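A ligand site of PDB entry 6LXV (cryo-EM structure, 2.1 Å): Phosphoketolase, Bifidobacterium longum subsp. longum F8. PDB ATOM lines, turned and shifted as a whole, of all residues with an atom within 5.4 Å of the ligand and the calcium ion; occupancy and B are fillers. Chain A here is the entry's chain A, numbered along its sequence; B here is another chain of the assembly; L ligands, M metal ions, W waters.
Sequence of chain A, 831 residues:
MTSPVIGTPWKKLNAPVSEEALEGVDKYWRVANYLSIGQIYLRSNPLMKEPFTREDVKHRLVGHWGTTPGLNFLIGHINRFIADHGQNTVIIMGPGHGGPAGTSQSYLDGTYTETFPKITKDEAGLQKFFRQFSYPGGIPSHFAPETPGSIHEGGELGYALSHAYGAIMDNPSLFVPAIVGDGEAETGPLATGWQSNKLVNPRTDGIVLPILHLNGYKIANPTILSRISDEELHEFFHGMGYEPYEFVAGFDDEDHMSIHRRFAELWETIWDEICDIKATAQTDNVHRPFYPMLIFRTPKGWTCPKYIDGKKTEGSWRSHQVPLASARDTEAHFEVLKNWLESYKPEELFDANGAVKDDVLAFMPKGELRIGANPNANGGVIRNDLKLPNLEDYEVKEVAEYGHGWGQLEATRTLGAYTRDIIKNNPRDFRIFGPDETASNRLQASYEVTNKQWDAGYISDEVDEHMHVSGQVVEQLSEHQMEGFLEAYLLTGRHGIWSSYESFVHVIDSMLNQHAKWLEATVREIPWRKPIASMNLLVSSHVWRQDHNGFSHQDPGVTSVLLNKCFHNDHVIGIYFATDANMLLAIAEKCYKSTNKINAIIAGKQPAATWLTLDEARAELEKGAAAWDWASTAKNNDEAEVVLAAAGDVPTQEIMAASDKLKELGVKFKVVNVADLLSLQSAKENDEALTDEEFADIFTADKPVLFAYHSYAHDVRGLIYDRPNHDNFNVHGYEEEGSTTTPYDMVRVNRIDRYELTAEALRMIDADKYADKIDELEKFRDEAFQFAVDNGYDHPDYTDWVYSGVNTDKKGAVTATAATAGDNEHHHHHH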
ATOM      1  N   GLY A  66     -12.026  21.969  -4.570  1.00  0.00           N
ATOM      2  CA  GLY A  66     -10.791  21.209  -4.439  1.00  0.00           C
ATOM      3  C   GLY A  66      -9.633  21.978  -3.830  1.00  0.00           C
ATOM      4  O   GLY A  66      -9.107  21.594  -2.806  1.00  0.00           O
ATOM      5  N   THR A  67      -9.371  23.160  -4.339  1.00  0.00           N
ATOM      6  CA  THR A  67      -8.351  24.021  -3.772  1.00  0.00           C
ATOM      7  C   THR A  67      -8.747  24.644  -2.415  1.00  0.00           C
ATOM      8  O   THR A  67      -7.864  24.970  -1.662  1.00  0.00           O
ATOM      9  CB  THR A  67      -8.005  25.111  -4.805  1.00  0.00           C
ATOM     10  OG1 THR A  67      -6.824  25.767  -4.409  1.00  0.00           O
ATOM     11  CG2 THR A  67      -9.112  26.139  -4.959  1.00  0.00           C
ATOM     12  N   PRO A  95      -4.658  30.091  -7.179  1.00  0.00           N
ATOM     13  CA  PRO A  95      -5.867  29.334  -7.579  1.00  0.00           C
ATOM     14  C   PRO A  95      -7.117  30.145  -7.266  1.00  0.00           C
ATOM     15  O   PRO A  95      -7.805  29.943  -6.317  1.00  0.00           O
ATOM     16  CB  PRO A  95      -5.763  28.064  -6.727  1.00  0.00           C
ATOM     17  CG  PRO A  95      -4.467  28.126  -6.082  1.00  0.00           C
ATOM     18  CD  PRO A  95      -4.150  29.532  -5.936  1.00  0.00           C
ATOM     19  N   HIS A  97     -10.009  30.491  -8.474  1.00  0.00           N
ATOM     20  CA  HIS A  97     -11.245  29.758  -8.368  1.00  0.00           C
ATOM     21  C   HIS A  97     -11.518  29.243  -6.959  1.00  0.00           C
ATOM     22  O   HIS A  97     -12.595  28.728  -6.743  1.00  0.00           O
ATOM     23  CB  HIS A  97     -11.262  28.586  -9.338  1.00  0.00           C
ATOM     24  CG  HIS A  97     -10.125  27.630  -9.158  1.00  0.00           C
ATOM     25  ND1 HIS A  97      -8.842  27.900  -9.541  1.00  0.00           N
ATOM     26  CD2 HIS A  97     -10.084  26.414  -8.572  1.00  0.00           C
ATOM     27  CE1 HIS A  97      -8.076  26.884  -9.249  1.00  0.00           C
ATOM     28  NE2 HIS A  97      -8.802  25.969  -8.678  1.00  0.00           N
ATOM     29  N   GLY A 155      -8.253  34.022 -12.332  1.00  0.00           N
ATOM     30  CA  GLY A 155      -9.133  33.275 -13.205  1.00  0.00           C
ATOM     31  C   GLY A 155      -8.339  32.602 -14.293  1.00  0.00           C
ATOM     32  O   GLY A 155      -8.212  31.392 -14.342  1.00  0.00           O
ATOM     33  N   GLU A 156      -7.725  33.410 -15.108  1.00  0.00           N
ATOM     34  CA  GLU A 156      -6.678  32.952 -15.986  1.00  0.00           C
ATOM     35  C   GLU A 156      -5.383  32.698 -15.208  1.00  0.00           C
ATOM     36  O   GLU A 156      -4.850  33.593 -14.596  1.00  0.00           O
ATOM     37  CB  GLU A 156      -6.447  33.988 -17.056  1.00  0.00           C
ATOM     38  CG  GLU A 156      -5.632  33.566 -18.161  1.00  0.00           C
ATOM     39  CD  GLU A 156      -5.673  34.583 -19.250  1.00  0.00           C
ATOM     40  OE1 GLU A 156      -6.768  34.903 -19.712  1.00  0.00           O
ATOM     41  OE2 GLU A 156      -4.605  35.100 -19.595  1.00  0.00           O
ATOM     42  N   LEU A 157      -4.845  31.519 -15.335  1.00  0.00           N
ATOM     43  CA  LEU A 157      -3.772  31.088 -14.437  1.00  0.00           C
ATOM     44  C   LEU A 157      -2.387  31.411 -14.963  1.00  0.00           C
ATOM     45  O   LEU A 157      -2.169  31.490 -16.158  1.00  0.00           O
ATOM     46  CB  LEU A 157      -3.918  29.602 -14.201  1.00  0.00           C
ATOM     47  CG  LEU A 157      -5.158  29.188 -13.431  1.00  0.00           C
ATOM     48  CD1 LEU A 157      -5.212  27.696 -13.464  1.00  0.00           C
ATOM     49  CD2 LEU A 157      -5.192  29.686 -12.020  1.00  0.00           C
ATOM     50  N   GLY A 181      -1.042  27.420  -7.542  1.00  0.00           N
ATOM     51  CA  GLY A 181      -1.564  26.141  -8.008  1.00  0.00           C
ATOM     52  C   GLY A 181      -0.530  25.167  -8.547  1.00  0.00           C
ATOM     53  O   GLY A 181       0.378  25.636  -9.185  1.00  0.00           O
ATOM     54  N   ASP A 182      -0.585  23.870  -8.287  1.00  0.00           N
ATOM     55  CA  ASP A 182       0.436  23.059  -8.915  1.00  0.00           C
ATOM     56  C   ASP A 182       0.140  22.798 -10.390  1.00  0.00           C
ATOM     57  O   ASP A 182       1.062  22.624 -11.143  1.00  0.00           O
ATOM     58  CB  ASP A 182       0.734  21.743  -8.167  1.00  0.00           C
ATOM     59  CG  ASP A 182      -0.445  20.807  -7.969  1.00  0.00           C
ATOM     60  OD1 ASP A 182      -1.502  21.162  -8.181  1.00  0.00           O
ATOM     61  OD2 ASP A 182      -0.287  19.673  -7.622  1.00  0.00           O
ATOM     62  N   GLY A 183      -1.122  22.868 -10.787  1.00  0.00           N
ATOM     63  CA  GLY A 183      -1.472  22.983 -12.175  1.00  0.00           C
ATOM     64  C   GLY A 183      -1.070  24.316 -12.766  1.00  0.00           C
ATOM     65  O   GLY A 183      -0.504  24.362 -13.830  1.00  0.00           O
ATOM     66  N   GLU A 184      -1.292  25.390 -12.042  1.00  0.00           N
ATOM     67  CA  GLU A 184      -0.886  26.711 -12.492  1.00  0.00           C
ATOM     68  C   GLU A 184       0.623  26.807 -12.725  1.00  0.00           C
ATOM     69  O   GLU A 184       1.063  27.477 -13.633  1.00  0.00           O
ATOM     70  CB  GLU A 184      -1.327  27.769 -11.478  1.00  0.00           C
ATOM     71  CG  GLU A 184      -0.764  29.199 -11.716  1.00  0.00           C
ATOM     72  CD  GLU A 184      -1.233  30.260 -10.686  1.00  0.00           C
ATOM     73  OE1 GLU A 184      -1.490  29.926  -9.523  1.00  0.00           O
ATOM     74  OE2 GLU A 184      -1.347  31.416 -11.046  1.00  0.00           O
ATOM     75  N   ALA A 185       1.421  26.101 -11.940  1.00  0.00           N
ATOM     76  CA  ALA A 185       2.841  26.003 -12.169  1.00  0.00           C
ATOM     77  C   ALA A 185       3.249  25.332 -13.493  1.00  0.00           C
ATOM     78  O   ALA A 185       4.375  25.491 -13.914  1.00  0.00           O
ATOM     79  CB  ALA A 185       3.461  25.292 -11.008  1.00  0.00           C
ATOM     80  N   THR A 187       1.956  26.425 -16.331  1.00  0.00           N
ATOM     81  CA  THR A 187       1.815  27.395 -17.399  1.00  0.00           C
ATOM     82  C   THR A 187       3.146  28.065 -17.720  1.00  0.00           C
ATOM     83  O   THR A 187       4.079  28.070 -16.934  1.00  0.00           O
ATOM     84  CB  THR A 187       0.774  28.482 -17.105  1.00  0.00           C
ATOM     85  OG1 THR A 187       1.219  29.316 -16.042  1.00  0.00           O
ATOM     86  CG2 THR A 187      -0.550  27.959 -16.769  1.00  0.00           C
ATOM     87  N   HIS A 213       0.946  25.101  -3.898  1.00  0.00           N
ATOM     88  CA  HIS A 213      -0.243  24.349  -3.460  1.00  0.00           C
ATOM     89  C   HIS A 213      -0.275  22.993  -4.169  1.00  0.00           C
ATOM     90  O   HIS A 213      -1.046  22.740  -5.076  1.00  0.00           O
ATOM     91  CB  HIS A 213      -1.466  25.206  -3.733  1.00  0.00           C
ATOM     92  CG  HIS A 213      -2.734  24.724  -3.111  1.00  0.00           C
ATOM     93  ND1 HIS A 213      -2.814  23.681  -2.220  1.00  0.00           N
ATOM     94  CD2 HIS A 213      -3.992  25.151  -3.293  1.00  0.00           C
ATOM     95  CE1 HIS A 213      -4.055  23.529  -1.853  1.00  0.00           C
ATOM     96  NE2 HIS A 213      -4.792  24.412  -2.486  1.00  0.00           N
ATOM     97  N   ASN A 215      -1.368  20.007  -4.415  1.00  0.00           N
ATOM     98  CA  ASN A 215      -2.419  19.103  -4.004  1.00  0.00           C
ATOM     99  C   ASN A 215      -2.496  17.901  -4.932  1.00  0.00           C
ATOM    100  O   ASN A 215      -3.337  17.080  -4.760  1.00  0.00           O
ATOM    101  CB  ASN A 215      -3.770  19.847  -3.790  1.00  0.00           C
ATOM    102  CG  ASN A 215      -4.306  20.563  -5.007  1.00  0.00           C
ATOM    103  OD1 ASN A 215      -3.910  20.271  -6.045  1.00  0.00           O
ATOM    104  ND2 ASN A 215      -5.121  21.540  -4.840  1.00  0.00           N
ATOM    105  N   GLY A 216      -1.663  17.833  -5.946  1.00  0.00           N
ATOM    106  CA  GLY A 216      -1.510  16.675  -6.768  1.00  0.00           C
ATOM    107  C   GLY A 216      -2.266  16.651  -8.071  1.00  0.00           C
ATOM    108  O   GLY A 216      -2.001  15.798  -8.863  1.00  0.00           O
ATOM    109  N   TYR A 217      -3.237  17.542  -8.271  1.00  0.00           N
ATOM    110  CA  TYR A 217      -4.273  17.471  -9.293  1.00  0.00           C
ATOM    111  C   TYR A 217      -4.583  18.881  -9.753  1.00  0.00           C
ATOM    112  O   TYR A 217      -4.409  19.841  -9.041  1.00  0.00           O
ATOM    113  CB  TYR A 217      -5.564  16.666  -8.871  1.00  0.00           C
ATOM    114  CG  TYR A 217      -5.213  15.266  -8.571  1.00  0.00           C
ATOM    115  CD1 TYR A 217      -4.926  14.916  -7.261  1.00  0.00           C
ATOM    116  CD2 TYR A 217      -5.036  14.310  -9.579  1.00  0.00           C
ATOM    117  CE1 TYR A 217      -4.470  13.785  -6.974  1.00  0.00           C
ATOM    118  CE2 TYR A 217      -4.602  13.118  -9.266  1.00  0.00           C
ATOM    119  CZ  TYR A 217      -4.327  12.848  -7.961  1.00  0.00           C
ATOM    120  OH  TYR A 217      -3.884  11.682  -7.549  1.00  0.00           O
ATOM    121  N   LYS A 218      -4.962  18.982 -10.997  1.00  0.00           N
ATOM    122  CA  LYS A 218      -5.564  20.074 -11.693  1.00  0.00           C
ATOM    123  C   LYS A 218      -7.001  19.596 -11.975  1.00  0.00           C
ATOM    124  O   LYS A 218      -7.599  19.024 -11.064  1.00  0.00           O
ATOM    125  CB  LYS A 218      -4.693  20.494 -12.873  1.00  0.00           C
ATOM    126  CG  LYS A 218      -4.170  19.481 -13.819  1.00  0.00           C
ATOM    127  CD  LYS A 218      -3.362  20.145 -14.946  1.00  0.00           C
ATOM    128  CE  LYS A 218      -2.885  19.135 -15.960  1.00  0.00           C
ATOM    129  NZ  LYS A 218      -1.775  18.311 -15.599  1.00  0.00           N
ATOM    130  N   ILE A 219      -7.633  20.007 -13.064  1.00  0.00           N
ATOM    131  CA  ILE A 219      -9.068  19.705 -13.269  1.00  0.00           C
ATOM    132  C   ILE A 219      -9.331  18.205 -13.329  1.00  0.00           C
ATOM    133  O   ILE A 219     -10.154  17.682 -12.608  1.00  0.00           O
ATOM    134  CB  ILE A 219      -9.643  20.377 -14.513  1.00  0.00           C
ATOM    135  CG1 ILE A 219      -9.627  21.891 -14.400  1.00  0.00           C
ATOM    136  CG2 ILE A 219     -11.064  19.840 -14.794  1.00  0.00           C
ATOM    137  CD1 ILE A 219     -10.204  22.502 -15.469  1.00  0.00           C
ATOM    138  N   THR A 223      -0.710  16.459 -11.577  1.00  0.00           N
ATOM    139  CA  THR A 223       0.163  17.555 -11.900  1.00  0.00           C
ATOM    140  C   THR A 223       1.573  17.010 -12.029  1.00  0.00           C
ATOM    141  O   THR A 223       1.952  16.140 -11.271  1.00  0.00           O
ATOM    142  CB  THR A 223       0.030  18.704 -10.864  1.00  0.00           C
ATOM    143  OG1 THR A 223       0.224  18.232  -9.535  1.00  0.00           O
ATOM    144  CG2 THR A 223      -1.338  19.414 -10.973  1.00  0.00           C
ATOM    145  N   LYS A 300      -6.089  16.945  -2.365  1.00  0.00           N
ATOM    146  CA  LYS A 300      -7.015  17.861  -2.997  1.00  0.00           C
ATOM    147  C   LYS A 300      -8.425  17.656  -2.446  1.00  0.00           C
ATOM    148  O   LYS A 300      -8.839  16.538  -2.216  1.00  0.00           O
ATOM    149  CB  LYS A 300      -7.000  17.736  -4.520  1.00  0.00           C
ATOM    150  CG  LYS A 300      -7.749  18.819  -5.176  1.00  0.00           C
ATOM    151  CD  LYS A 300      -7.641  18.826  -6.623  1.00  0.00           C
ATOM    152  CE  LYS A 300      -8.243  20.040  -7.179  1.00  0.00           C
ATOM    153  NZ  LYS A 300      -7.739  20.454  -8.468  1.00  0.00           N
ATOM    154  N   HIS A 320     -12.377  18.619  -7.676  1.00  0.00           N
ATOM    155  CA  HIS A 320     -11.975  19.920  -8.209  1.00  0.00           C
ATOM    156  C   HIS A 320     -13.111  20.941  -8.195  1.00  0.00           C
ATOM    157  O   HIS A 320     -12.999  22.004  -7.602  1.00  0.00           O
ATOM    158  CB  HIS A 320     -11.437  19.799  -9.629  1.00  0.00           C
ATOM    159  CG  HIS A 320     -11.117  21.115 -10.246  1.00  0.00           C
ATOM    160  ND1 HIS A 320     -10.064  21.870  -9.827  1.00  0.00           N
ATOM    161  CD2 HIS A 320     -11.785  21.862 -11.128  1.00  0.00           C
ATOM    162  CE1 HIS A 320     -10.051  23.005 -10.491  1.00  0.00           C
ATOM    163  NE2 HIS A 320     -11.074  23.002 -11.313  1.00  0.00           N
ATOM    164  N   PRO B 435      -5.406  21.731 -22.897  1.00  0.00           N
ATOM    165  CA  PRO B 435      -4.827  22.144 -21.632  1.00  0.00           C
ATOM    166  C   PRO B 435      -5.673  21.708 -20.443  1.00  0.00           C
ATOM    167  O   PRO B 435      -6.262  22.520 -19.785  1.00  0.00           O
ATOM    168  CB  PRO B 435      -4.753  23.651 -21.786  1.00  0.00           C
ATOM    169  CG  PRO B 435      -5.854  23.950 -22.643  1.00  0.00           C
ATOM    170  CD  PRO B 435      -5.972  22.885 -23.598  1.00  0.00           C
ATOM    171  N   ASP B 436      -5.698  20.395 -20.196  1.00  0.00           N
ATOM    172  CA  ASP B 436      -6.458  19.744 -19.114  1.00  0.00           C
ATOM    173  C   ASP B 436      -7.966  19.985 -19.327  1.00  0.00           C
ATOM    174  O   ASP B 436      -8.739  20.174 -18.417  1.00  0.00           O
ATOM    175  CB  ASP B 436      -5.867  20.208 -17.768  1.00  0.00           C
ATOM    176  CG  ASP B 436      -6.526  19.638 -16.540  1.00  0.00           C
ATOM    177  OD1 ASP B 436      -6.742  18.426 -16.338  1.00  0.00           O
ATOM    178  OD2 ASP B 436      -6.794  20.509 -15.781  1.00  0.00           O
ATOM    179  N   GLU B 437      -8.365  20.039 -20.572  1.00  0.00           N
ATOM    180  CA  GLU B 437      -9.736  20.381 -20.906  1.00  0.00           C
ATOM    181  C   GLU B 437     -10.392  19.416 -21.891  1.00  0.00           C
ATOM    182  O   GLU B 437     -11.482  19.704 -22.317  1.00  0.00           O
ATOM    183  CB  GLU B 437      -9.805  21.832 -21.450  1.00  0.00           C
ATOM    184  CG  GLU B 437      -9.641  22.923 -20.385  1.00  0.00           C
ATOM    185  CD  GLU B 437      -9.317  24.301 -20.954  1.00  0.00           C
ATOM    186  OE1 GLU B 437      -9.509  24.522 -22.116  1.00  0.00           O
ATOM    187  OE2 GLU B 437      -8.852  25.187 -20.236  1.00  0.00           O
ATOM    188  N   LEU B 477      -1.317  21.744 -18.575  1.00  0.00           N
ATOM    189  CA  LEU B 477      -1.974  23.023 -18.383  1.00  0.00           C
ATOM    190  C   LEU B 477      -1.062  24.166 -18.865  1.00  0.00           C
ATOM    191  O   LEU B 477      -0.398  24.850 -18.096  1.00  0.00           O
ATOM    192  CB  LEU B 477      -2.407  23.170 -16.937  1.00  0.00           C
ATOM    193  CG  LEU B 477      -3.042  24.455 -16.398  1.00  0.00           C
ATOM    194  CD1 LEU B 477      -3.905  25.160 -17.301  1.00  0.00           C
ATOM    195  CD2 LEU B 477      -3.559  24.366 -15.007  1.00  0.00           C
ATOM    196  N   GLU B 479      -1.522  26.427 -22.652  1.00  0.00           N
ATOM    197  CA  GLU B 479      -1.944  26.668 -24.024  1.00  0.00           C
ATOM    198  C   GLU B 479      -0.751  26.804 -24.961  1.00  0.00           C
ATOM    199  O   GLU B 479      -0.799  26.285 -26.052  1.00  0.00           O
ATOM    200  CB  GLU B 479      -2.875  27.894 -24.087  1.00  0.00           C
ATOM    201  CG  GLU B 479      -4.221  27.844 -23.337  1.00  0.00           C
ATOM    202  CD  GLU B 479      -4.176  27.894 -21.790  1.00  0.00           C
ATOM    203  OE1 GLU B 479      -3.228  28.379 -21.184  1.00  0.00           O
ATOM    204  OE2 GLU B 479      -5.125  27.419 -21.178  1.00  0.00           O
ATOM    205  N   TYR B 501     -10.991  26.280 -23.852  1.00  0.00           N
ATOM    206  CA  TYR B 501     -11.999  27.259 -23.532  1.00  0.00           C
ATOM    207  C   TYR B 501     -11.707  28.500 -24.320  1.00  0.00           C
ATOM    208  O   TYR B 501     -10.540  28.869 -24.486  1.00  0.00           O
ATOM    209  CB  TYR B 501     -12.017  27.608 -22.057  1.00  0.00           C
ATOM    210  CG  TYR B 501     -12.275  26.491 -21.131  1.00  0.00           C
ATOM    211  CD1 TYR B 501     -12.834  25.286 -21.543  1.00  0.00           C
ATOM    212  CD2 TYR B 501     -11.932  26.617 -19.824  1.00  0.00           C
ATOM    213  CE1 TYR B 501     -13.028  24.320 -20.700  1.00  0.00           C
ATOM    214  CE2 TYR B 501     -12.136  25.653 -18.951  1.00  0.00           C
ATOM    215  CZ  TYR B 501     -12.683  24.503 -19.382  1.00  0.00           C
ATOM    216  OH  TYR B 501     -12.862  23.543 -18.481  1.00  0.00           O
ATOM    217  N   PHE B 504      -9.497  31.524 -23.087  1.00  0.00           N
ATOM    218  CA  PHE B 504      -8.075  31.255 -22.973  1.00  0.00           C
ATOM    219  C   PHE B 504      -7.389  31.016 -24.299  1.00  0.00           C
ATOM    220  O   PHE B 504      -6.188  30.817 -24.291  1.00  0.00           O
ATOM    221  CB  PHE B 504      -7.819  30.074 -22.080  1.00  0.00           C
ATOM    222  CG  PHE B 504      -8.441  30.174 -20.722  1.00  0.00           C
ATOM    223  CD1 PHE B 504      -8.323  31.302 -19.957  1.00  0.00           C
ATOM    224  CD2 PHE B 504      -9.105  29.105 -20.180  1.00  0.00           C
ATOM    225  CE1 PHE B 504      -8.901  31.366 -18.697  1.00  0.00           C
ATOM    226  CE2 PHE B 504      -9.657  29.192 -18.946  1.00  0.00           C
ATOM    227  CZ  PHE B 504      -9.527  30.303 -18.192  1.00  0.00           C
ATOM    228  N   VAL B 507      -4.454  33.516 -24.784  1.00  0.00           N
ATOM    229  CA  VAL B 507      -3.139  33.098 -24.344  1.00  0.00           C
ATOM    230  C   VAL B 507      -2.194  32.816 -25.497  1.00  0.00           C
ATOM    231  O   VAL B 507      -1.038  33.168 -25.419  1.00  0.00           O
ATOM    232  CB  VAL B 507      -3.230  31.905 -23.360  1.00  0.00           C
ATOM    233  CG1 VAL B 507      -1.854  31.450 -22.918  1.00  0.00           C
ATOM    234  CG2 VAL B 507      -4.098  32.277 -22.166  1.00  0.00           C
ATOM    235  N   HIS B 553     -14.021  35.377 -17.344  1.00  0.00           N
ATOM    236  CA  HIS B 553     -13.810  34.284 -18.281  1.00  0.00           C
ATOM    237  C   HIS B 553     -14.592  34.460 -19.556  1.00  0.00           C
ATOM    238  O   HIS B 553     -14.704  33.531 -20.333  1.00  0.00           O
ATOM    239  CB  HIS B 553     -14.226  32.971 -17.691  1.00  0.00           C
ATOM    240  CG  HIS B 553     -13.401  32.536 -16.529  1.00  0.00           C
ATOM    241  ND1 HIS B 553     -13.437  33.184 -15.319  1.00  0.00           N
ATOM    242  CD2 HIS B 553     -12.621  31.458 -16.358  1.00  0.00           C
ATOM    243  CE1 HIS B 553     -12.637  32.564 -14.480  1.00  0.00           C
ATOM    244  NE2 HIS B 553     -12.114  31.526 -15.099  1.00  0.00           N
HETATM  245  N1  LIG L   1      -6.044  27.692 -18.648  1.00  0.00           N
HETATM  246  C1  LIG L   1      -5.688  28.860 -18.017  1.00  0.00           C
HETATM  247  C2  LIG L   1      -4.610  29.787 -18.527  1.00  0.00           C
HETATM  248  N2  LIG L   1      -6.337  29.147 -16.851  1.00  0.00           N
HETATM  249  C3  LIG L   1      -7.296  28.337 -16.342  1.00  0.00           C
HETATM  250  N3  LIG L   1      -7.911  28.703 -15.286  1.00  0.00           N
HETATM  251  C4  LIG L   1      -7.684  27.183 -17.011  1.00  0.00           C
HETATM  252  C5  LIG L   1      -7.010  26.880 -18.168  1.00  0.00           C
HETATM  253  C6  LIG L   1      -8.737  26.282 -16.454  1.00  0.00           C
HETATM  254  N4  LIG L   1      -8.479  25.815 -15.107  1.00  0.00           N
HETATM  255  C7  LIG L   1      -9.005  26.258 -13.913  1.00  0.00           C
HETATM  256  S1  LIG L   1      -8.654  25.589 -12.549  1.00  0.00           S
HETATM  257  C8  LIG L   1      -7.701  24.682 -13.443  1.00  0.00           C
HETATM  258  C9  LIG L   1      -7.666  24.885 -14.794  1.00  0.00           C
HETATM  259  C10 LIG L   1      -6.959  24.065 -15.803  1.00  0.00           C
HETATM  260  C11 LIG L   1      -6.928  23.706 -12.652  1.00  0.00           C
HETATM  261  C12 LIG L   1      -6.040  24.507 -11.776  1.00  0.00           C
HETATM  262  O1  LIG L   1      -5.072  23.738 -11.118  1.00  0.00           O
HETATM  263  P1  LIG L   1      -4.259  24.106  -9.881  1.00  0.00           P
HETATM  264  O2  LIG L   1      -3.413  25.125 -10.448  1.00  0.00           O
HETATM  265  O3  LIG L   1      -3.691  22.834  -9.913  1.00  0.00           O
HETATM  266  O4  LIG L   1      -5.480  24.494  -9.003  1.00  0.00           O
HETATM  267  P2  LIG L   1      -6.156  23.872  -7.748  1.00  0.00           P
HETATM  268  O5  LIG L   1      -5.880  22.544  -7.703  1.00  0.00           O
HETATM  269  O6  LIG L   1      -5.512  24.329  -6.574  1.00  0.00           O
HETATM  270  O7  LIG L   1      -7.581  23.830  -7.757  1.00  0.00           O
HETATM  271 CA    CA M   1      -3.738  21.649  -7.888  1.00  0.00          CA
HETATM  272  O   HOH W   1      -8.760  29.564 -12.051  1.00  0.00           O
HETATM  273  O   HOH W   2      -3.063  23.596  -6.658  1.00  0.00           O
HETATM  274  O   HOH W   3     -10.780  29.831 -13.961  1.00  0.00           O
HETATM  275  O   HOH W   4     -10.343  23.394  -7.200  1.00  0.00           O
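An oxygen (O2) of the ligand sits at hydrogen-bond distance from the backbone NH of Glu 184, 2.7 Å away.
The backbone NH (N) of Gly 183 sits at hydrogen-bond distance from an oxygen (O2) of the ligand (3.2 Å).
N2 of the ligand lies within hydrogen-bond range of N of Leu 157 (3.2 Å).
An oxygen (O7) of the ligand sits at hydrogen-bond distance from a ring nitrogen (NE2) of His 97, 2.6 Å away.
OG1 of Thr 67 is in hydrogen-bond range of O6 of the ligand (2.9 Å).
The backbone carbonyl oxygen (O) of Gly 155 lies within hydrogen-bond range of a nitrogen (N3) of the ligand, at 2.9 Å.
The side-chain carboxylate (OE2) of Glu 479 of chain B sits at hydrogen-bond distance from a nitrogen (N1) of the ligand (2.7 Å).
A ring nitrogen (NE2) of His 320 sits close to a sulfur (S1) of the ligand.
The side-chain amino group (NZ) of Lys 300 lies within salt-bridge range of an oxygen (O7) of the ligand, at 3.5 Å.
The backbone carbonyl oxygen (O) of His 320 lies within hydrogen-bond range of the backbone NH (N) of Gly 66 (3.2 Å).
The side-chain carboxylate (OD2) of Asp 182 is in hydrogen-bond range of the backbone NH (N) of Gly 216, 2.8 Å away.
The side-chain carboxylate (OE1) of Glu 437 of chain B sits at hydrogen-bond distance from the backbone NH (N) of Tyr 501 of chain B (2.9 Å).
NZ of Lys 300 sits at hydrogen-bond distance from O of Lys 218, 3.0 Å away.
The backbone carbonyl oxygen (O) of Glu 184 sits at hydrogen-bond distance from the side-chain hydroxyl (OG1) of Thr 187, at 3.0 Å.
The backbone NH of Ile 219 sits at hydrogen-bond distance from the side-chain carboxylate of Asp 436 of chain B (2.9 Å).
The side-chain carboxylate (OD2) of Asp 182 lies within hydrogen-bond range of the side-chain hydroxyl (OG1) of Thr 223 (2.4 Å).
The backbone NH (N) of Asp 182 sits at hydrogen-bond distance from the backbone carbonyl oxygen (O) of His 213, 3.4 Å away.
Residues that only touch the ligand: Gly 181 (3.2 Å), Glu 437 of chain B (3.2 Å), Phe 504 of chain B (3.4 Å), Leu 477 of chain B (3.5 Å), Ile 219 (3.5 Å), Asp 436 of chain B (3.6 Å), Lys 218 (3.7 Å), His 213 (3.7 Å), Pro 95 (3.7 Å) and Glu 156 (3.9 Å).
Hydrophobic or aromatic side chains within 4 Å of the ligand: Pro 95, His 97, Leu 157, His 213, Ile 219, His 320, Leu 477 of chain B and Phe 504 of chain B.
Within 4 Å of the ligand: Thr 67, Pro 95, His 97, Gly 155, Glu 156, Leu 157, Gly 181, Asp 182, Gly 183, Glu 184, His 213, Asn 215, Tyr 217, Lys 218, Ile 219, Lys 300, His 320, Asp 436 of chain B, Glu 437 of chain B, Leu 477 of chain B, Glu 479 of chain B and Phe 504 of chain B.
The nearest printed residue that does not touch the ligand is Tyr 501 of chain B (4.3 Å).
Within 4 Å of the calcium ion: Asp 182, Asn 215 and Tyr 217.
The nearest printed residue that does not touch the calcium ion is His 213 (4.04 Å).
O of Tyr 217 is bound to the calcium ion.
The calcium ion is bound by OD1 of Asp 182.
OD1 of Asn 215 is bound to the calcium ion.
An oxygen (O5) of the ligand binds the calcium ion (2.3 Å).
The calcium ion is bound by O3 of the ligand (2.3 Å).
Water W2 binds the calcium ion (2.4 Å).
The calcium ion has six donor atoms within binding distance.
Water W2 lies within hydrogen-bond range of an oxygen (O6) of the ligand (2.6 Å), the backbone carbonyl oxygen (O) of His 213 (2.7 Å), the backbone NH (N) of Asp 182 (3.0 Å) and the side-chain amide nitrogen (ND2) of Asn 215 (3.4 Å).
Water W4 lies within hydrogen-bond range of O7 of the ligand (2.9 Å), O of His 320 (3.0 Å), N of Thr 67 (3.0 Å), NE2 of His 97 (3.3 Å) and N of Gly 66 (3.4 Å).
Water W3 lies within hydrogen-bond range of a ring nitrogen (NE2) of His 553 of chain B (2.4 Å), the backbone carbonyl oxygen of Gly 155 (3.0 Å) and a nitrogen (N3) of the ligand (3.4 Å).
Water W1 lies within hydrogen-bond range of the backbone carbonyl oxygen of Gly 155 (3.0 Å), a ring nitrogen (ND1) of His 97 (3.0 Å) and a nitrogen (N3) of the ligand (3.5 Å).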
